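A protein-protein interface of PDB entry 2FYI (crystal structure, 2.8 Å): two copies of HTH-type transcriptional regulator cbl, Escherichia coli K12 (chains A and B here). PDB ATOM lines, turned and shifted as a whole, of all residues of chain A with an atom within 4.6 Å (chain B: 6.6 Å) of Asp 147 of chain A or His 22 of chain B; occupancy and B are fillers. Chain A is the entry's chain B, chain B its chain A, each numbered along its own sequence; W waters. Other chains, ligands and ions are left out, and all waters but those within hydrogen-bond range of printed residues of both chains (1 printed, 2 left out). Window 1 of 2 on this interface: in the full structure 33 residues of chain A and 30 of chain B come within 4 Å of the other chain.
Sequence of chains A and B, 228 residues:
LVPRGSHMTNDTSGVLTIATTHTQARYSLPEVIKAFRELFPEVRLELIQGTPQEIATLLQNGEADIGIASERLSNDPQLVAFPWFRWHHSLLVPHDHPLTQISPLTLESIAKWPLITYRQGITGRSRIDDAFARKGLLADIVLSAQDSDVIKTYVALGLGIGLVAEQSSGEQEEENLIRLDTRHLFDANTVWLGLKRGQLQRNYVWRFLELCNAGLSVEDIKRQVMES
Water W1 bridges the side-chain amide nitrogen (NE2) of Gln 146 of chain A (3.2 Å) and the backbone carbonyl oxygen (O) of Gln 146 of chain B (3.5 Å).
Hydrophobic or aromatic side chains of chain A within 4 Å of the printed part of chain B: His 22, Ala 145 and Val 150. Printed residues of chain B that touch a printed residue of chain A: His 22, Arg 26, Gln 49, Gly 50, Asp 147, Asp 149 and Val 150. Hydrophobic or aromatic side chains of chain B within 4 Å of the printed part of chain A: His 22 and Val 150.
Asp 147 of chain B touches His 22 of chain A (OD1 to CD2, 3.2 Å). His 22 of chain A touches Val 150 of chain B (CD2 to CG2, 3.6 Å). Ala 145 of chain A touches Gln 49 of chain B (CA to OE1, 3.4 Å). NE2 of Gln 146 of chain A touches CA of Gly 50 of chain B (3.6 Å). His 22 of chain B touches Asp 147 of chain A (CD2 to OD1, 2.9 Å). Asp 149 of chain A touches Asp 149 of chain B. CD2 of His 22 of chain B touches CG2 of Val 150 of chain A, 3.7 Å away. OE1 of Gln 49 of chain B touches CG2 of Val 150 of chain A, at 3.4 Å.
The backbone NH (N) of Gly 50 of chain B lies within hydrogen-bond range of the backbone carbonyl oxygen (O) of Thr 20 of chain B, 2.8 Å away. NE2 of His 22 of chain B lies within hydrogen-bond range of OD2 of Asp 149 of chain B, 2.8 Å away. The side-chain carboxylate of Asp 149 of chain B lies within salt-bridge range of the guanidinium group of Arg 26 of chain B (2.7 Å). The side-chain hydroxyl (OH) of Tyr 27 of chain B is in hydrogen-bond range of the side-chain carboxylate (OD1) of Asp 149 of chain B, 3.4 Å away. OD2 of Asp 147 of chain B lies within hydrogen-bond range of N of Val 150 of chain B (3.1 Å). OD2 of Asp 147 of chain A sits at hydrogen-bond distance from N of Val 150 of chain A, at 3.0 Å.
His 22 of chain A touches Asp 147 of chain B, and with the chains exchanged Asp 147 of chain A touches His 22 of chain B. His 22 of chain A touches Val 150 of chain B, and with the chains exchanged Val 150 of chain A touches His 22 of chain B. Asp 149 of chain A touches its own counterpart, Asp 149 of chain B. Of the 11 pairs that touch across the chains among the printed residues, 5 have their exchanged pair printed and touching as well.
OD2 of Asp 149 of chain A is in salt-bridge range of NH1 of Arg 26 of chain B. The side-chain amide oxygen (OE1) of Gln 49 of chain B lies within hydrogen-bond range of the backbone NH (N) of Gln 146 of chain A. NE2 of Gln 49 of chain B lies within hydrogen-bond range of OD1 of Asp 147 of chain A.
Asp 147 of chain A touches just these residues of chain B: His 22 and Gln 49. Of chain A, only Asp 147 (2.9 Å) and Val 150 (3.7 Å) come within 4 Å of His 22 of chain B. Of the printed residues of chain B, Ala 145 of chain A touches Gln 49 (3.4 Å). Printed residues of chain A within 4 Å of Val 150 of chain B: His 22. Of the printed residues of chain B, Asp 149 of chain A touches Arg 26 and Asp 149. Of the printed residues of chain A, Arg 26 of chain B touches Asp 149. Of the printed residues of chain B, Gln 146 of chain A touches Gln 49 (2.7 Å) and Gly 50 (3.6 Å). Thr 23 of chain B touches none of the printed residues of chain A. Gln 24 of chain B touches none of the printed residues of chain A. The nearest residue of chain B that does not touch Asp 147 of chain A is Asp 147 of chain B (4.1 Å). The nearest residue of chain A that does not touch His 22 of chain B is Asp 149 of chain A (4.3 Å). The nearest printed residue of chain A that does not touch Asp 149 of chain B is His 22 of chain A (4.4 Å).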
ATOM      1  N   HIS A  22       9.391  22.516  28.840  1.00  0.00           N
ATOM      2  CA  HIS A  22       8.575  23.706  29.029  1.00  0.00           C
ATOM      3  C   HIS A  22       8.559  24.143  30.494  1.00  0.00           C
ATOM      4  O   HIS A  22       8.728  25.337  30.789  1.00  0.00           O
ATOM      5  CB  HIS A  22       7.165  23.430  28.517  1.00  0.00           C
ATOM      6  CG  HIS A  22       6.186  24.509  28.831  1.00  0.00           C
ATOM      7  ND1 HIS A  22       5.544  24.596  30.052  1.00  0.00           N
ATOM      8  CD2 HIS A  22       5.741  25.555  28.092  1.00  0.00           C
ATOM      9  CE1 HIS A  22       4.769  25.671  30.061  1.00  0.00           C
ATOM     10  NE2 HIS A  22       4.865  26.265  28.880  1.00  0.00           N
ATOM     11  N   TYR A 118      -0.773  16.271  32.681  1.00  0.00           N
ATOM     12  CA  TYR A 118       0.269  15.939  31.700  1.00  0.00           C
ATOM     13  C   TYR A 118       0.130  14.525  31.105  1.00  0.00           C
ATOM     14  O   TYR A 118      -0.272  13.566  31.800  1.00  0.00           O
ATOM     15  CB  TYR A 118       1.637  16.068  32.353  1.00  0.00           C
ATOM     16  CG  TYR A 118       1.853  17.376  33.078  1.00  0.00           C
ATOM     17  CD1 TYR A 118       1.874  17.430  34.476  1.00  0.00           C
ATOM     18  CD2 TYR A 118       2.014  18.575  32.367  1.00  0.00           C
ATOM     19  CE1 TYR A 118       2.057  18.620  35.129  1.00  0.00           C
ATOM     20  CE2 TYR A 118       2.205  19.766  33.005  1.00  0.00           C
ATOM     21  CZ  TYR A 118       2.231  19.786  34.384  1.00  0.00           C
ATOM     22  OH  TYR A 118       2.435  20.993  35.034  1.00  0.00           O
ATOM     23  N   ALA A 145      -2.060  17.104  28.433  1.00  0.00           N
ATOM     24  CA  ALA A 145      -1.308  18.249  27.977  1.00  0.00           C
ATOM     25  C   ALA A 145       0.148  17.889  27.901  1.00  0.00           C
ATOM     26  O   ALA A 145       0.592  16.977  28.621  1.00  0.00           O
ATOM     27  CB  ALA A 145      -1.493  19.401  28.955  1.00  0.00           C
ATOM     28  N   GLN A 146       0.890  18.618  27.056  1.00  0.00           N
ATOM     29  CA  GLN A 146       2.363  18.616  27.156  1.00  0.00           C
ATOM     30  C   GLN A 146       2.896  19.811  27.909  1.00  0.00           C
ATOM     31  O   GLN A 146       4.109  19.945  27.971  1.00  0.00           O
ATOM     32  CB  GLN A 146       3.084  18.520  25.810  1.00  0.00           C
ATOM     33  CG  GLN A 146       2.358  17.672  24.806  1.00  0.00           C
ATOM     34  CD  GLN A 146       2.918  17.829  23.394  1.00  0.00           C
ATOM     35  OE1 GLN A 146       3.596  16.925  22.908  1.00  0.00           O
ATOM     36  NE2 GLN A 146       2.640  18.973  22.728  1.00  0.00           N
ATOM     37  N   ASP A 147       2.029  20.675  28.452  1.00  0.00           N
ATOM     38  CA  ASP A 147       2.510  21.840  29.223  1.00  0.00           C
ATOM     39  C   ASP A 147       1.480  22.497  30.144  1.00  0.00           C
ATOM     40  O   ASP A 147       0.296  22.338  29.961  1.00  0.00           O
ATOM     41  CB  ASP A 147       3.164  22.881  28.305  1.00  0.00           C
ATOM     42  CG  ASP A 147       2.166  23.598  27.426  1.00  0.00           C
ATOM     43  OD1 ASP A 147       2.236  23.446  26.181  1.00  0.00           O
ATOM     44  OD2 ASP A 147       1.310  24.332  27.967  1.00  0.00           O
ATOM     45  N   SER A 148       1.931  23.241  31.138  1.00  0.00           N
ATOM     46  CA  SER A 148       1.044  23.717  32.187  1.00  0.00           C
ATOM     47  C   SER A 148       0.136  24.817  31.702  1.00  0.00           C
ATOM     48  O   SER A 148      -0.891  25.080  32.287  1.00  0.00           O
ATOM     49  CB  SER A 148       1.862  24.226  33.368  1.00  0.00           C
ATOM     50  OG  SER A 148       2.931  23.330  33.691  1.00  0.00           O
ATOM     51  N   ASP A 149       0.509  25.468  30.618  1.00  0.00           N
ATOM     52  CA  ASP A 149      -0.262  26.593  30.118  1.00  0.00           C
ATOM     53  C   ASP A 149      -1.556  26.175  29.457  1.00  0.00           C
ATOM     54  O   ASP A 149      -2.582  26.839  29.601  1.00  0.00           O
ATOM     55  CB  ASP A 149       0.604  27.416  29.172  1.00  0.00           C
ATOM     56  CG  ASP A 149       1.522  28.361  29.939  1.00  0.00           C
ATOM     57  OD1 ASP A 149       2.796  28.295  29.799  1.00  0.00           O
ATOM     58  OD2 ASP A 149       0.940  29.133  30.754  1.00  0.00           O
ATOM     59  N   VAL A 150      -1.501  25.073  28.714  1.00  0.00           N
ATOM     60  CA  VAL A 150      -2.693  24.467  28.158  1.00  0.00           C
ATOM     61  C   VAL A 150      -3.624  24.045  29.295  1.00  0.00           C
ATOM     62  O   VAL A 150      -4.829  24.319  29.252  1.00  0.00           O
ATOM     63  CB  VAL A 150      -2.339  23.289  27.226  1.00  0.00           C
ATOM     64  CG1 VAL A 150      -3.569  22.608  26.719  1.00  0.00           C
ATOM     65  CG2 VAL A 150      -1.523  23.799  26.062  1.00  0.00           C
ATOM     66  N   ILE A 151      -3.071  23.418  30.325  1.00  0.00           N
ATOM     67  CA  ILE A 151      -3.862  23.067  31.461  1.00  0.00           C
ATOM     68  C   ILE A 151      -4.616  24.253  32.032  1.00  0.00           C
ATOM     69  O   ILE A 151      -5.833  24.148  32.249  1.00  0.00           O
ATOM     70  CB  ILE A 151      -3.031  22.471  32.548  1.00  0.00           C
ATOM     71  CG1 ILE A 151      -2.357  21.185  32.053  1.00  0.00           C
ATOM     72  CG2 ILE A 151      -3.897  22.187  33.750  1.00  0.00           C
ATOM     73  CD1 ILE A 151      -1.445  20.526  33.077  1.00  0.00           C
ATOM     74  N   THR B  20      -4.581  18.056  19.081  1.00  0.00           N
ATOM     75  CA  THR B  20      -4.177  19.356  18.626  1.00  0.00           C
ATOM     76  C   THR B  20      -2.835  19.851  19.181  1.00  0.00           C
ATOM     77  O   THR B  20      -2.220  19.219  20.033  1.00  0.00           O
ATOM     78  CB  THR B  20      -5.265  20.351  18.943  1.00  0.00           C
ATOM     79  OG1 THR B  20      -5.042  21.515  18.162  1.00  0.00           O
ATOM     80  CG2 THR B  20      -5.285  20.706  20.416  1.00  0.00           C
ATOM     81  N   THR B  21      -2.391  20.996  18.690  1.00  0.00           N
ATOM     82  CA  THR B  21      -1.145  21.644  19.134  1.00  0.00           C
ATOM     83  C   THR B  21      -1.380  22.704  20.193  1.00  0.00           C
ATOM     84  O   THR B  21      -2.512  23.151  20.390  1.00  0.00           O
ATOM     85  CB  THR B  21      -0.467  22.368  17.952  1.00  0.00           C
ATOM     86  OG1 THR B  21      -1.390  23.314  17.358  1.00  0.00           O
ATOM     87  CG2 THR B  21      -0.060  21.360  16.914  1.00  0.00           C
ATOM     88  N   HIS B  22      -0.300  23.129  20.836  1.00  0.00           N
ATOM     89  CA  HIS B  22      -0.342  24.159  21.853  1.00  0.00           C
ATOM     90  C   HIS B  22      -1.028  25.394  21.320  1.00  0.00           C
ATOM     91  O   HIS B  22      -1.883  26.006  21.986  1.00  0.00           O
ATOM     92  CB  HIS B  22       1.086  24.516  22.257  1.00  0.00           C
ATOM     93  CG  HIS B  22       1.167  25.652  23.231  1.00  0.00           C
ATOM     94  ND1 HIS B  22       1.120  26.978  22.839  1.00  0.00           N
ATOM     95  CD2 HIS B  22       1.280  25.657  24.581  1.00  0.00           C
ATOM     96  CE1 HIS B  22       1.196  27.747  23.909  1.00  0.00           C
ATOM     97  NE2 HIS B  22       1.289  26.970  24.977  1.00  0.00           N
ATOM     98  N   THR B  23      -0.653  25.757  20.097  1.00  0.00           N
ATOM     99  CA  THR B  23      -1.171  26.978  19.505  1.00  0.00           C
ATOM    100  C   THR B  23      -2.702  27.019  19.481  1.00  0.00           C
ATOM    101  O   THR B  23      -3.300  27.980  19.943  1.00  0.00           O
ATOM    102  CB  THR B  23      -0.673  27.236  18.053  1.00  0.00           C
ATOM    103  OG1 THR B  23       0.738  27.023  17.940  1.00  0.00           O
ATOM    104  CG2 THR B  23      -0.996  28.653  17.660  1.00  0.00           C
ATOM    105  N   GLN B  24      -3.354  26.001  18.923  1.00  0.00           N
ATOM    106  CA  GLN B  24      -4.806  26.103  18.812  1.00  0.00           C
ATOM    107  C   GLN B  24      -5.446  25.815  20.165  1.00  0.00           C
ATOM    108  O   GLN B  24      -6.402  26.468  20.530  1.00  0.00           O
ATOM    109  CB  GLN B  24      -5.391  25.242  17.668  1.00  0.00           C
ATOM    110  CG  GLN B  24      -4.362  24.539  16.748  1.00  0.00           C
ATOM    111  CD  GLN B  24      -3.565  25.472  15.821  1.00  0.00           C
ATOM    112  OE1 GLN B  24      -3.756  26.701  15.790  1.00  0.00           O
ATOM    113  NE2 GLN B  24      -2.660  24.876  15.050  1.00  0.00           N
ATOM    114  N   ALA B  25      -4.886  24.893  20.932  1.00  0.00           N
ATOM    115  CA  ALA B  25      -5.446  24.609  22.214  1.00  0.00           C
ATOM    116  C   ALA B  25      -5.597  25.905  23.041  1.00  0.00           C
ATOM    117  O   ALA B  25      -6.606  26.111  23.734  1.00  0.00           O
ATOM    118  CB  ALA B  25      -4.601  23.597  22.898  1.00  0.00           C
ATOM    119  N   ARG B  26      -4.623  26.799  22.937  1.00  0.00           N
ATOM    120  CA  ARG B  26      -4.673  28.006  23.722  1.00  0.00           C
ATOM    121  C   ARG B  26      -5.406  29.157  23.085  1.00  0.00           C
ATOM    122  O   ARG B  26      -6.073  29.925  23.765  1.00  0.00           O
ATOM    123  CB  ARG B  26      -3.271  28.489  24.010  1.00  0.00           C
ATOM    124  CG  ARG B  26      -2.526  27.525  24.831  1.00  0.00           C
ATOM    125  CD  ARG B  26      -1.683  28.211  25.787  1.00  0.00           C
ATOM    126  NE  ARG B  26      -2.461  28.872  26.809  1.00  0.00           N
ATOM    127  CZ  ARG B  26      -1.940  29.843  27.552  1.00  0.00           C
ATOM    128  NH1 ARG B  26      -0.676  30.221  27.341  1.00  0.00           N
ATOM    129  NH2 ARG B  26      -2.657  30.425  28.498  1.00  0.00           N
ATOM    130  N   TYR B  27      -5.260  29.326  21.785  1.00  0.00           N
ATOM    131  CA  TYR B  27      -5.631  30.599  21.196  1.00  0.00           C
ATOM    132  C   TYR B  27      -6.824  30.594  20.260  1.00  0.00           C
ATOM    133  O   TYR B  27      -7.312  31.648  19.867  1.00  0.00           O
ATOM    134  CB  TYR B  27      -4.447  31.228  20.477  1.00  0.00           C
ATOM    135  CG  TYR B  27      -3.236  31.294  21.343  1.00  0.00           C
ATOM    136  CD1 TYR B  27      -2.049  30.661  20.976  1.00  0.00           C
ATOM    137  CD2 TYR B  27      -3.288  31.956  22.556  1.00  0.00           C
ATOM    138  CE1 TYR B  27      -0.937  30.691  21.791  1.00  0.00           C
ATOM    139  CE2 TYR B  27      -2.194  32.004  23.370  1.00  0.00           C
ATOM    140  CZ  TYR B  27      -1.017  31.365  22.994  1.00  0.00           C
ATOM    141  OH  TYR B  27       0.073  31.447  23.847  1.00  0.00           O
ATOM    142  N   GLN B  49      -2.915  16.886  23.527  1.00  0.00           N
ATOM    143  CA  GLN B  49      -1.983  17.821  22.929  1.00  0.00           C
ATOM    144  C   GLN B  49      -0.781  17.079  22.388  1.00  0.00           C
ATOM    145  O   GLN B  49      -0.239  16.208  23.050  1.00  0.00           O
ATOM    146  CB  GLN B  49      -1.501  18.824  23.958  1.00  0.00           C
ATOM    147  CG  GLN B  49      -0.445  19.809  23.445  1.00  0.00           C
ATOM    148  CD  GLN B  49       0.041  20.722  24.561  1.00  0.00           C
ATOM    149  OE1 GLN B  49      -0.398  20.588  25.715  1.00  0.00           O
ATOM    150  NE2 GLN B  49       0.940  21.638  24.242  1.00  0.00           N
ATOM    151  N   GLY B  50      -0.340  17.421  21.187  1.00  0.00           N
ATOM    152  CA  GLY B  50       0.794  16.724  20.634  1.00  0.00           C
ATOM    153  C   GLY B  50       1.396  17.478  19.489  1.00  0.00           C
ATOM    154  O   GLY B  50       0.911  18.540  19.145  1.00  0.00           O
ATOM    155  N   GLN B 146       8.956  24.840  21.388  1.00  0.00           N
ATOM    156  CA  GLN B 146       7.788  24.069  21.044  1.00  0.00           C
ATOM    157  C   GLN B 146       6.490  24.849  21.154  1.00  0.00           C
ATOM    158  O   GLN B 146       5.473  24.362  20.697  1.00  0.00           O
ATOM    159  CB  GLN B 146       7.699  22.827  21.890  1.00  0.00           C
ATOM    160  CG  GLN B 146       8.177  21.670  21.152  1.00  0.00           C
ATOM    161  CD  GLN B 146       8.847  20.673  22.036  1.00  0.00           C
ATOM    162  OE1 GLN B 146       8.354  20.328  23.124  1.00  0.00           O
ATOM    163  NE2 GLN B 146       9.999  20.183  21.581  1.00  0.00           N
ATOM    164  N   ASP B 147       6.511  26.051  21.736  1.00  0.00           N
ATOM    165  CA  ASP B 147       5.279  26.838  21.897  1.00  0.00           C
ATOM    166  C   ASP B 147       5.493  28.332  22.182  1.00  0.00           C
ATOM    167  O   ASP B 147       6.579  28.758  22.527  1.00  0.00           O
ATOM    168  CB  ASP B 147       4.447  26.219  23.001  1.00  0.00           C
ATOM    169  CG  ASP B 147       5.094  26.374  24.367  1.00  0.00           C
ATOM    170  OD1 ASP B 147       5.624  25.350  24.897  1.00  0.00           O
ATOM    171  OD2 ASP B 147       5.086  27.529  24.905  1.00  0.00           O
ATOM    172  N   SER B 148       4.449  29.128  22.067  1.00  0.00           N
ATOM    173  CA  SER B 148       4.594  30.575  22.187  1.00  0.00           C
ATOM    174  C   SER B 148       4.817  31.115  23.584  1.00  0.00           C
ATOM    175  O   SER B 148       5.190  32.247  23.719  1.00  0.00           O
ATOM    176  CB  SER B 148       3.374  31.277  21.597  1.00  0.00           C
ATOM    177  OG  SER B 148       2.974  30.666  20.357  1.00  0.00           O
ATOM    178  N   ASP B 149       4.580  30.341  24.634  1.00  0.00           N
ATOM    179  CA  ASP B 149       4.724  30.888  25.986  1.00  0.00           C
ATOM    180  C   ASP B 149       6.174  30.877  26.414  1.00  0.00           C
ATOM    181  O   ASP B 149       6.649  31.817  27.067  1.00  0.00           O
ATOM    182  CB  ASP B 149       3.848  30.144  26.976  1.00  0.00           C
ATOM    183  CG  ASP B 149       2.364  30.323  26.668  1.00  0.00           C
ATOM    184  OD1 ASP B 149       1.864  31.482  26.679  1.00  0.00           O
ATOM    185  OD2 ASP B 149       1.673  29.313  26.377  1.00  0.00           O
ATOM    186  N   VAL B 150       6.887  29.818  26.029  1.00  0.00           N
ATOM    187  CA  VAL B 150       8.320  29.814  26.189  1.00  0.00           C
ATOM    188  C   VAL B 150       8.910  31.043  25.459  1.00  0.00           C
ATOM    189  O   VAL B 150       9.654  31.838  26.060  1.00  0.00           O
ATOM    190  CB  VAL B 150       8.915  28.495  25.714  1.00  0.00           C
ATOM    191  CG1 VAL B 150      10.435  28.556  25.699  1.00  0.00           C
ATOM    192  CG2 VAL B 150       8.472  27.417  26.611  1.00  0.00           C
HETATM  193  O   HOH W   1       4.068  21.820  22.623  1.00  0.00           O
